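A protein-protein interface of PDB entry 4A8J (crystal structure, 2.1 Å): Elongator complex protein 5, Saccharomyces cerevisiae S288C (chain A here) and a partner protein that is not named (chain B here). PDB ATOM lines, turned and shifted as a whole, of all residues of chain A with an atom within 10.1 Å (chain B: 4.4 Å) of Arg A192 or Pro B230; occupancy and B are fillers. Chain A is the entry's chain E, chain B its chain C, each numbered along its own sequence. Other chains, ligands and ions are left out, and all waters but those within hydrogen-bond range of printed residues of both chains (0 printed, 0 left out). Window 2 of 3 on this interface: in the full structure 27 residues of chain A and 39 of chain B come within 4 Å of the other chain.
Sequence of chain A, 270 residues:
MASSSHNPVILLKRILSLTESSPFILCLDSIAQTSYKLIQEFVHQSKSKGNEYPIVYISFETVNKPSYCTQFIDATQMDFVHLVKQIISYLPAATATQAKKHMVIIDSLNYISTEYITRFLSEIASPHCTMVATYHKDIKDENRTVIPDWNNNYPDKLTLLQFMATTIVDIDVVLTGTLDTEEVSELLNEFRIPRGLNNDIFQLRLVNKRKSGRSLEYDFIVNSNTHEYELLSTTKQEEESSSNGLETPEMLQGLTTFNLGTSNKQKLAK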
ATOM      1  N   ILE A  31      19.513 -28.423  16.842  1.00  0.00           N
ATOM      2  CA  ILE A  31      20.202 -29.173  17.898  1.00  0.00           C
ATOM      3  C   ILE A  31      19.246 -29.959  18.799  1.00  0.00           C
ATOM      4  O   ILE A  31      19.635 -30.978  19.387  1.00  0.00           O
ATOM      5  CB  ILE A  31      21.165 -28.304  18.721  1.00  0.00           C
ATOM      6  CG1 ILE A  31      20.416 -27.166  19.408  1.00  0.00           C
ATOM      7  CG2 ILE A  31      22.260 -27.742  17.811  1.00  0.00           C
ATOM      8  CD1 ILE A  31      21.311 -26.394  20.425  1.00  0.00           C
ATOM      9  N   LEU A 179       9.196 -28.845  30.972  1.00  0.00           N
ATOM     10  CA  LEU A 179       9.516 -27.594  30.293  1.00  0.00           C
ATOM     11  C   LEU A 179       8.657 -27.472  29.041  1.00  0.00           C
ATOM     12  O   LEU A 179       8.526 -28.430  28.275  1.00  0.00           O
ATOM     13  CB  LEU A 179      10.990 -27.565  29.896  1.00  0.00           C
ATOM     14  CG  LEU A 179      12.035 -27.634  31.008  1.00  0.00           C
ATOM     15  CD1 LEU A 179      13.403 -27.943  30.432  1.00  0.00           C
ATOM     16  CD2 LEU A 179      12.071 -26.340  31.797  1.00  0.00           C
ATOM     17  N   GLU A 182       8.804 -22.661  24.882  1.00  0.00           N
ATOM     18  CA  GLU A 182       9.508 -21.391  25.007  1.00  0.00           C
ATOM     19  C   GLU A 182      10.580 -21.424  26.099  1.00  0.00           C
ATOM     20  O   GLU A 182      11.634 -20.790  25.959  1.00  0.00           O
ATOM     21  CB  GLU A 182       8.529 -20.229  25.207  1.00  0.00           C
ATOM     22  N   GLU A 183      10.320 -22.173  27.171  1.00  0.00           N
ATOM     23  CA  GLU A 183      11.326 -22.376  28.215  1.00  0.00           C
ATOM     24  C   GLU A 183      12.562 -23.066  27.637  1.00  0.00           C
ATOM     25  O   GLU A 183      13.716 -22.679  27.904  1.00  0.00           O
ATOM     26  CB  GLU A 183      10.758 -23.221  29.358  1.00  0.00           C
ATOM     27  CG  GLU A 183       9.909 -22.466  30.366  1.00  0.00           C
ATOM     28  CD  GLU A 183       9.082 -23.396  31.246  1.00  0.00           C
ATOM     29  OE1 GLU A 183       8.693 -24.490  30.766  1.00  0.00           O
ATOM     30  OE2 GLU A 183       8.818 -23.036  32.415  1.00  0.00           O
ATOM     31  N   VAL A 184      12.315 -24.100  26.846  1.00  0.00           N
ATOM     32  CA  VAL A 184      13.406 -24.844  26.231  1.00  0.00           C
ATOM     33  C   VAL A 184      14.123 -23.926  25.250  1.00  0.00           C
ATOM     34  O   VAL A 184      15.345 -23.997  25.073  1.00  0.00           O
ATOM     35  CB  VAL A 184      12.910 -26.094  25.494  1.00  0.00           C
ATOM     36  CG1 VAL A 184      13.973 -26.574  24.508  1.00  0.00           C
ATOM     37  CG2 VAL A 184      12.542 -27.195  26.490  1.00  0.00           C
ATOM     38  N   SER A 185      13.355 -23.044  24.629  1.00  0.00           N
ATOM     39  CA  SER A 185      13.928 -22.055  23.731  1.00  0.00           C
ATOM     40  C   SER A 185      14.939 -21.147  24.424  1.00  0.00           C
ATOM     41  O   SER A 185      16.059 -20.962  23.932  1.00  0.00           O
ATOM     42  CB  SER A 185      12.822 -21.215  23.085  1.00  0.00           C
ATOM     43  OG  SER A 185      12.508 -21.739  21.809  1.00  0.00           O
ATOM     44  N   GLU A 186      14.554 -20.568  25.559  1.00  0.00           N
ATOM     45  CA  GLU A 186      15.482 -19.686  26.267  1.00  0.00           C
ATOM     46  C   GLU A 186      16.695 -20.437  26.852  1.00  0.00           C
ATOM     47  O   GLU A 186      17.844 -19.931  26.835  1.00  0.00           O
ATOM     48  CB  GLU A 186      14.756 -18.864  27.333  1.00  0.00           C
ATOM     49  CG  GLU A 186      13.642 -19.600  28.041  1.00  0.00           C
ATOM     50  CD  GLU A 186      12.800 -18.686  28.924  1.00  0.00           C
ATOM     51  OE1 GLU A 186      12.445 -17.570  28.466  1.00  0.00           O
ATOM     52  OE2 GLU A 186      12.498 -19.089  30.074  1.00  0.00           O
ATOM     53  N   LEU A 187      16.447 -21.649  27.349  1.00  0.00           N
ATOM     54  CA  LEU A 187      17.546 -22.473  27.820  1.00  0.00           C
ATOM     55  C   LEU A 187      18.540 -22.711  26.672  1.00  0.00           C
ATOM     56  O   LEU A 187      19.746 -22.488  26.827  1.00  0.00           O
ATOM     57  CB  LEU A 187      17.035 -23.808  28.367  1.00  0.00           C
ATOM     58  CG  LEU A 187      16.394 -23.741  29.753  1.00  0.00           C
ATOM     59  CD1 LEU A 187      15.856 -25.111  30.147  1.00  0.00           C
ATOM     60  CD2 LEU A 187      17.392 -23.237  30.791  1.00  0.00           C
ATOM     61  N   LEU A 188      18.039 -23.155  25.520  1.00  0.00           N
ATOM     62  CA  LEU A 188      18.908 -23.409  24.367  1.00  0.00           C
ATOM     63  C   LEU A 188      19.641 -22.118  23.935  1.00  0.00           C
ATOM     64  O   LEU A 188      20.794 -22.165  23.487  1.00  0.00           O
ATOM     65  CB  LEU A 188      18.121 -24.014  23.199  1.00  0.00           C
ATOM     66  CG  LEU A 188      17.561 -25.433  23.335  1.00  0.00           C
ATOM     67  CD1 LEU A 188      16.751 -25.826  22.082  1.00  0.00           C
ATOM     68  CD2 LEU A 188      18.668 -26.454  23.612  1.00  0.00           C
ATOM     69  N   ASN A 189      18.992 -20.969  24.105  1.00  0.00           N
ATOM     70  CA  ASN A 189      19.648 -19.688  23.814  1.00  0.00           C
ATOM     71  C   ASN A 189      20.814 -19.399  24.740  1.00  0.00           C
ATOM     72  O   ASN A 189      21.732 -18.681  24.367  1.00  0.00           O
ATOM     73  CB  ASN A 189      18.672 -18.503  23.856  1.00  0.00           C
ATOM     74  CG  ASN A 189      17.703 -18.505  22.689  1.00  0.00           C
ATOM     75  OD1 ASN A 189      17.951 -19.141  21.658  1.00  0.00           O
ATOM     76  ND2 ASN A 189      16.591 -17.789  22.844  1.00  0.00           N
ATOM     77  N   GLU A 190      20.765 -19.930  25.956  1.00  0.00           N
ATOM     78  CA  GLU A 190      21.901 -19.772  26.871  1.00  0.00           C
ATOM     79  C   GLU A 190      22.875 -20.962  26.825  1.00  0.00           C
ATOM     80  O   GLU A 190      23.810 -21.047  27.631  1.00  0.00           O
ATOM     81  CB  GLU A 190      21.406 -19.584  28.305  1.00  0.00           C
ATOM     82  CG  GLU A 190      20.644 -18.290  28.566  1.00  0.00           C
ATOM     83  CD  GLU A 190      20.134 -18.203  29.997  1.00  0.00           C
ATOM     84  OE1 GLU A 190      19.409 -19.137  30.426  1.00  0.00           O
ATOM     85  OE2 GLU A 190      20.473 -17.212  30.688  1.00  0.00           O
ATOM     86  N   PHE A 191      22.649 -21.870  25.888  1.00  0.00           N
ATOM     87  CA  PHE A 191      23.351 -23.167  25.829  1.00  0.00           C
ATOM     88  C   PHE A 191      23.326 -23.969  27.136  1.00  0.00           C
ATOM     89  O   PHE A 191      24.254 -24.731  27.450  1.00  0.00           O
ATOM     90  CB  PHE A 191      24.780 -23.039  25.283  1.00  0.00           C
ATOM     91  CG  PHE A 191      25.140 -24.124  24.309  1.00  0.00           C
ATOM     92  CD1 PHE A 191      24.773 -24.027  22.979  1.00  0.00           C
ATOM     93  CD2 PHE A 191      25.817 -25.265  24.731  1.00  0.00           C
ATOM     94  CE1 PHE A 191      25.076 -25.043  22.070  1.00  0.00           C
ATOM     95  CE2 PHE A 191      26.124 -26.286  23.827  1.00  0.00           C
ATOM     96  CZ  PHE A 191      25.763 -26.166  22.495  1.00  0.00           C
ATOM     97  N   ARG A 192      22.259 -23.790  27.902  1.00  0.00           N
ATOM     98  CA  ARG A 192      21.976 -24.666  29.032  1.00  0.00           C
ATOM     99  C   ARG A 192      21.103 -25.807  28.512  1.00  0.00           C
ATOM    100  O   ARG A 192      19.887 -25.777  28.673  1.00  0.00           O
ATOM    101  CB  ARG A 192      21.225 -23.880  30.106  1.00  0.00           C
ATOM    102  CG  ARG A 192      22.073 -22.859  30.867  1.00  0.00           C
ATOM    103  CD  ARG A 192      21.155 -21.959  31.666  1.00  0.00           C
ATOM    104  NE  ARG A 192      21.860 -20.989  32.491  1.00  0.00           N
ATOM    105  CZ  ARG A 192      22.303 -21.257  33.712  1.00  0.00           C
ATOM    106  NH1 ARG A 192      22.114 -22.467  34.222  1.00  0.00           N
ATOM    107  NH2 ARG A 192      22.932 -20.326  34.413  1.00  0.00           N
ATOM    108  N   ILE A 193      21.724 -26.788  27.861  1.00  0.00           N
ATOM    109  CA  ILE A 193      20.990 -27.852  27.190  1.00  0.00           C
ATOM    110  C   ILE A 193      20.209 -28.694  28.193  1.00  0.00           C
ATOM    111  O   ILE A 193      20.788 -29.272  29.110  1.00  0.00           O
ATOM    112  CB  ILE A 193      21.944 -28.791  26.430  1.00  0.00           C
ATOM    113  CG1 ILE A 193      22.939 -27.968  25.602  1.00  0.00           C
ATOM    114  CG2 ILE A 193      21.156 -29.766  25.557  1.00  0.00           C
ATOM    115  CD1 ILE A 193      22.286 -27.076  24.571  1.00  0.00           C
ATOM    116  N   PRO A 194      18.889 -28.773  28.010  1.00  0.00           N
ATOM    117  CA  PRO A 194      18.043 -29.532  28.936  1.00  0.00           C
ATOM    118  C   PRO A 194      18.005 -31.022  28.596  1.00  0.00           C
ATOM    119  O   PRO A 194      18.411 -31.437  27.508  1.00  0.00           O
ATOM    120  CB  PRO A 194      16.664 -28.917  28.718  1.00  0.00           C
ATOM    121  CG  PRO A 194      16.682 -28.487  27.273  1.00  0.00           C
ATOM    122  CD  PRO A 194      18.105 -28.101  26.956  1.00  0.00           C
ATOM    123  N   ARG A 195      17.538 -31.822  29.547  1.00  0.00           N
ATOM    124  CA  ARG A 195      17.256 -33.232  29.310  1.00  0.00           C
ATOM    125  C   ARG A 195      15.977 -33.298  28.486  1.00  0.00           C
ATOM    126  O   ARG A 195      15.237 -32.313  28.426  1.00  0.00           O
ATOM    127  CB  ARG A 195      17.087 -33.946  30.653  1.00  0.00           C
ATOM    128  CG  ARG A 195      18.359 -33.931  31.530  1.00  0.00           C
ATOM    129  CD  ARG A 195      18.102 -34.361  32.979  1.00  0.00           C
ATOM    130  NE  ARG A 195      17.549 -33.271  33.781  1.00  0.00           N
ATOM    131  CZ  ARG A 195      17.213 -33.370  35.065  1.00  0.00           C
ATOM    132  NH1 ARG A 195      17.373 -34.527  35.710  1.00  0.00           N
ATOM    133  NH2 ARG A 195      16.711 -32.312  35.697  1.00  0.00           N
ATOM    134  N   GLY A 196      15.723 -34.429  27.837  1.00  0.00           N
ATOM    135  CA  GLY A 196      14.463 -34.620  27.147  1.00  0.00           C
ATOM    136  C   GLY A 196      14.423 -34.285  25.660  1.00  0.00           C
ATOM    137  O   GLY A 196      13.330 -34.173  25.082  1.00  0.00           O
ATOM    138  N   LEU A 197      15.595 -34.142  25.038  1.00  0.00           N
ATOM    139  CA  LEU A 197      15.667 -33.799  23.615  1.00  0.00           C
ATOM    140  C   LEU A 197      16.243 -34.973  22.834  1.00  0.00           C
ATOM    141  O   LEU A 197      16.655 -35.978  23.411  1.00  0.00           O
ATOM    142  CB  LEU A 197      16.520 -32.539  23.394  1.00  0.00           C
ATOM    143  CG  LEU A 197      16.236 -31.314  24.276  1.00  0.00           C
ATOM    144  CD1 LEU A 197      17.145 -30.134  23.915  1.00  0.00           C
ATOM    145  CD2 LEU A 197      14.771 -30.907  24.200  1.00  0.00           C
ATOM    146  N   GLN B  44      30.324 -22.202  31.775  1.00  0.00           N
ATOM    147  CA  GLN B  44      30.533 -20.760  31.910  1.00  0.00           C
ATOM    148  C   GLN B  44      31.823 -20.511  32.677  1.00  0.00           C
ATOM    149  O   GLN B  44      32.346 -21.414  33.318  1.00  0.00           O
ATOM    150  CB  GLN B  44      29.329 -20.074  32.563  1.00  0.00           C
ATOM    151  CG  GLN B  44      28.022 -20.302  31.794  1.00  0.00           C
ATOM    152  CD  GLN B  44      26.881 -19.429  32.297  1.00  0.00           C
ATOM    153  OE1 GLN B  44      27.084 -18.273  32.655  1.00  0.00           O
ATOM    154  NE2 GLN B  44      25.673 -19.981  32.323  1.00  0.00           N
ATOM    155  N   CYS B  46      32.541 -18.780  35.287  1.00  0.00           N
ATOM    156  CA  CYS B  46      32.465 -18.880  36.748  1.00  0.00           C
ATOM    157  C   CYS B  46      32.316 -20.321  37.268  1.00  0.00           C
ATOM    158  O   CYS B  46      32.424 -20.555  38.465  1.00  0.00           O
ATOM    159  CB  CYS B  46      31.321 -18.035  37.287  1.00  0.00           C
ATOM    160  SG  CYS B  46      29.746 -18.526  36.630  1.00  0.00           S
ATOM    161  N   THR B  47      32.049 -21.280  36.377  1.00  0.00           N
ATOM    162  CA  THR B  47      32.043 -22.700  36.758  1.00  0.00           C
ATOM    163  C   THR B  47      33.008 -23.498  35.889  1.00  0.00           C
ATOM    164  O   THR B  47      32.595 -24.252  34.995  1.00  0.00           O
ATOM    165  CB  THR B  47      30.612 -23.306  36.676  1.00  0.00           C
ATOM    166  OG1 THR B  47      30.080 -23.078  35.365  1.00  0.00           O
ATOM    167  CG2 THR B  47      29.684 -22.623  37.691  1.00  0.00           C
ATOM    168  N   ASN B 198      25.789 -16.096  27.251  1.00  0.00           N
ATOM    169  CA  ASN B 198      25.237 -15.628  28.509  1.00  0.00           C
ATOM    170  C   ASN B 198      25.442 -14.144  28.783  1.00  0.00           C
ATOM    171  O   ASN B 198      25.553 -13.727  29.937  1.00  0.00           O
ATOM    172  CB  ASN B 198      25.810 -16.461  29.648  1.00  0.00           C
ATOM    173  CG  ASN B 198      25.239 -17.849  29.668  1.00  0.00           C
ATOM    174  OD1 ASN B 198      24.163 -18.072  30.222  1.00  0.00           O
ATOM    175  ND2 ASN B 198      25.934 -18.794  29.030  1.00  0.00           N
ATOM    176  N   ASN B 229      27.055 -25.133  34.812  1.00  0.00           N
ATOM    177  CA  ASN B 229      26.558 -23.762  34.889  1.00  0.00           C
ATOM    178  C   ASN B 229      26.331 -23.349  36.326  1.00  0.00           C
ATOM    179  O   ASN B 229      26.037 -24.199  37.168  1.00  0.00           O
ATOM    180  CB  ASN B 229      25.238 -23.656  34.105  1.00  0.00           C
ATOM    181  CG  ASN B 229      25.433 -23.778  32.598  1.00  0.00           C
ATOM    182  OD1 ASN B 229      25.808 -22.813  31.932  1.00  0.00           O
ATOM    183  ND2 ASN B 229      25.167 -24.949  32.058  1.00  0.00           N
ATOM    184  N   PRO B 230      26.436 -22.042  36.617  1.00  0.00           N
ATOM    185  CA  PRO B 230      26.025 -21.584  37.950  1.00  0.00           C
ATOM    186  C   PRO B 230      24.509 -21.734  38.054  1.00  0.00           C
ATOM    187  O   PRO B 230      23.827 -21.807  37.017  1.00  0.00           O
ATOM    188  CB  PRO B 230      26.402 -20.096  37.941  1.00  0.00           C
ATOM    189  CG  PRO B 230      26.321 -19.699  36.451  1.00  0.00           C
ATOM    190  CD  PRO B 230      26.849 -20.925  35.738  1.00  0.00           C
ATOM    191  N   LEU B 231      23.976 -21.777  39.272  1.00  0.00           N
ATOM    192  CA  LEU B 231      22.520 -21.807  39.432  1.00  0.00           C
ATOM    193  C   LEU B 231      21.917 -20.422  39.158  1.00  0.00           C
ATOM    194  O   LEU B 231      22.553 -19.404  39.445  1.00  0.00           O
ATOM    195  CB  LEU B 231      22.141 -22.276  40.836  1.00  0.00           C
ATOM    196  CG  LEU B 231      22.718 -23.612  41.317  1.00  0.00           C
ATOM    197  CD1 LEU B 231      21.996 -24.067  42.569  1.00  0.00           C
ATOM    198  CD2 LEU B 231      22.620 -24.668  40.240  1.00  0.00           C
ATOM    199  N   LYS B 232      20.701 -20.394  38.609  1.00  0.00           N
ATOM    200  CA  LYS B 232      19.982 -19.140  38.347  1.00  0.00           C
ATOM    201  C   LYS B 232      19.171 -18.704  39.556  1.00  0.00           C
ATOM    202  O   LYS B 232      18.710 -17.563  39.647  1.00  0.00           O
ATOM    203  CB  LYS B 232      19.005 -19.316  37.184  1.00  0.00           C
ATOM    204  CG  LYS B 232      19.629 -19.614  35.847  1.00  0.00           C
ATOM    205  CD  LYS B 232      18.672 -20.452  35.021  1.00  0.00           C
ATOM    206  CE  LYS B 232      18.768 -20.139  33.536  1.00  0.00           C
ATOM    207  NZ  LYS B 232      18.295 -18.757  33.249  1.00  0.00           N
ATOM    208  N   THR B 240      28.316 -24.986  44.172  1.00  0.00           N
ATOM    209  CA  THR B 240      29.032 -24.251  43.137  1.00  0.00           C
ATOM    210  C   THR B 240      28.118 -24.064  41.931  1.00  0.00           C
ATOM    211  O   THR B 240      27.944 -22.957  41.440  1.00  0.00           O
ATOM    212  CB  THR B 240      30.301 -24.989  42.718  1.00  0.00           C
ATOM    213  OG1 THR B 240      31.161 -25.111  43.843  1.00  0.00           O
ATOM    214  CG2 THR B 240      31.039 -24.245  41.639  1.00  0.00           C
ATOM    215  N   GLY B 241      27.517 -25.151  41.468  1.00  0.00           N
ATOM    216  CA  GLY B 241      26.666 -25.083  40.291  1.00  0.00           C
ATOM    217  C   GLY B 241      26.040 -26.426  39.965  1.00  0.00           C
ATOM    218  O   GLY B 241      25.966 -27.323  40.814  1.00  0.00           O
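O of Glu A190 sits at hydrogen-bond distance from ND2 of Asn B198, 3.4 Å away. NZ of Lys B232 lies within salt-bridge range of OE1 of Glu A190 (3.1 Å). NE2 of Gln B44 sits close to NH2 of Arg A192 (3.5 Å). The backbone carbonyl oxygen of Pro B230 sits at hydrogen-bond distance from the guanidinium group of Arg A192 (3.1 Å).
Of the 18 printed residues of chain A, 2 touch a printed residue of chain B. Among the printed residues, 6 pairs touch across the chains.
Asn B229 touches Arg A192. Arg A192 touches Lys B232.
Asn A189 touches none of the printed residues of chain B. Printed residues of chain B within 4 Å of Glu A190: Asn B198 (3.4 Å) and Lys B232 (3.1 Å). Arg A192 touches four residues of chain B. Gln B44 touches one residue of chain A. Of the printed residues of chain A, Asn B198 touches Glu A190 (3.4 Å). Pro B230 touches just one residue of chain A: Arg A192. The nearest residue of chain A that does not touch Pro B230 is Glu A190 (8.4 Å). The nearest printed residue of chain B that does not touch Glu A190 is Asn B229 (5.1 Å).
The backbone carbonyl oxygen of Leu A187 lies within hydrogen-bond range of the backbone NH of Arg A192 (3.0 Å). OE1 of Glu A190 is in salt-bridge range of NE of Arg A192, 3.7 Å away. The backbone carbonyl oxygen (O) of Gln B44 lies close to the side-chain hydroxyl (OG1) of Thr B47, at 3.5 Å. NE2 of Gln B44 lies within hydrogen-bond range of OD1 of Asn B198, 3.2 Å away. The side-chain amide nitrogen of Gln B44 lies within hydrogen-bond range of the side-chain amide oxygen of Asn B229.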
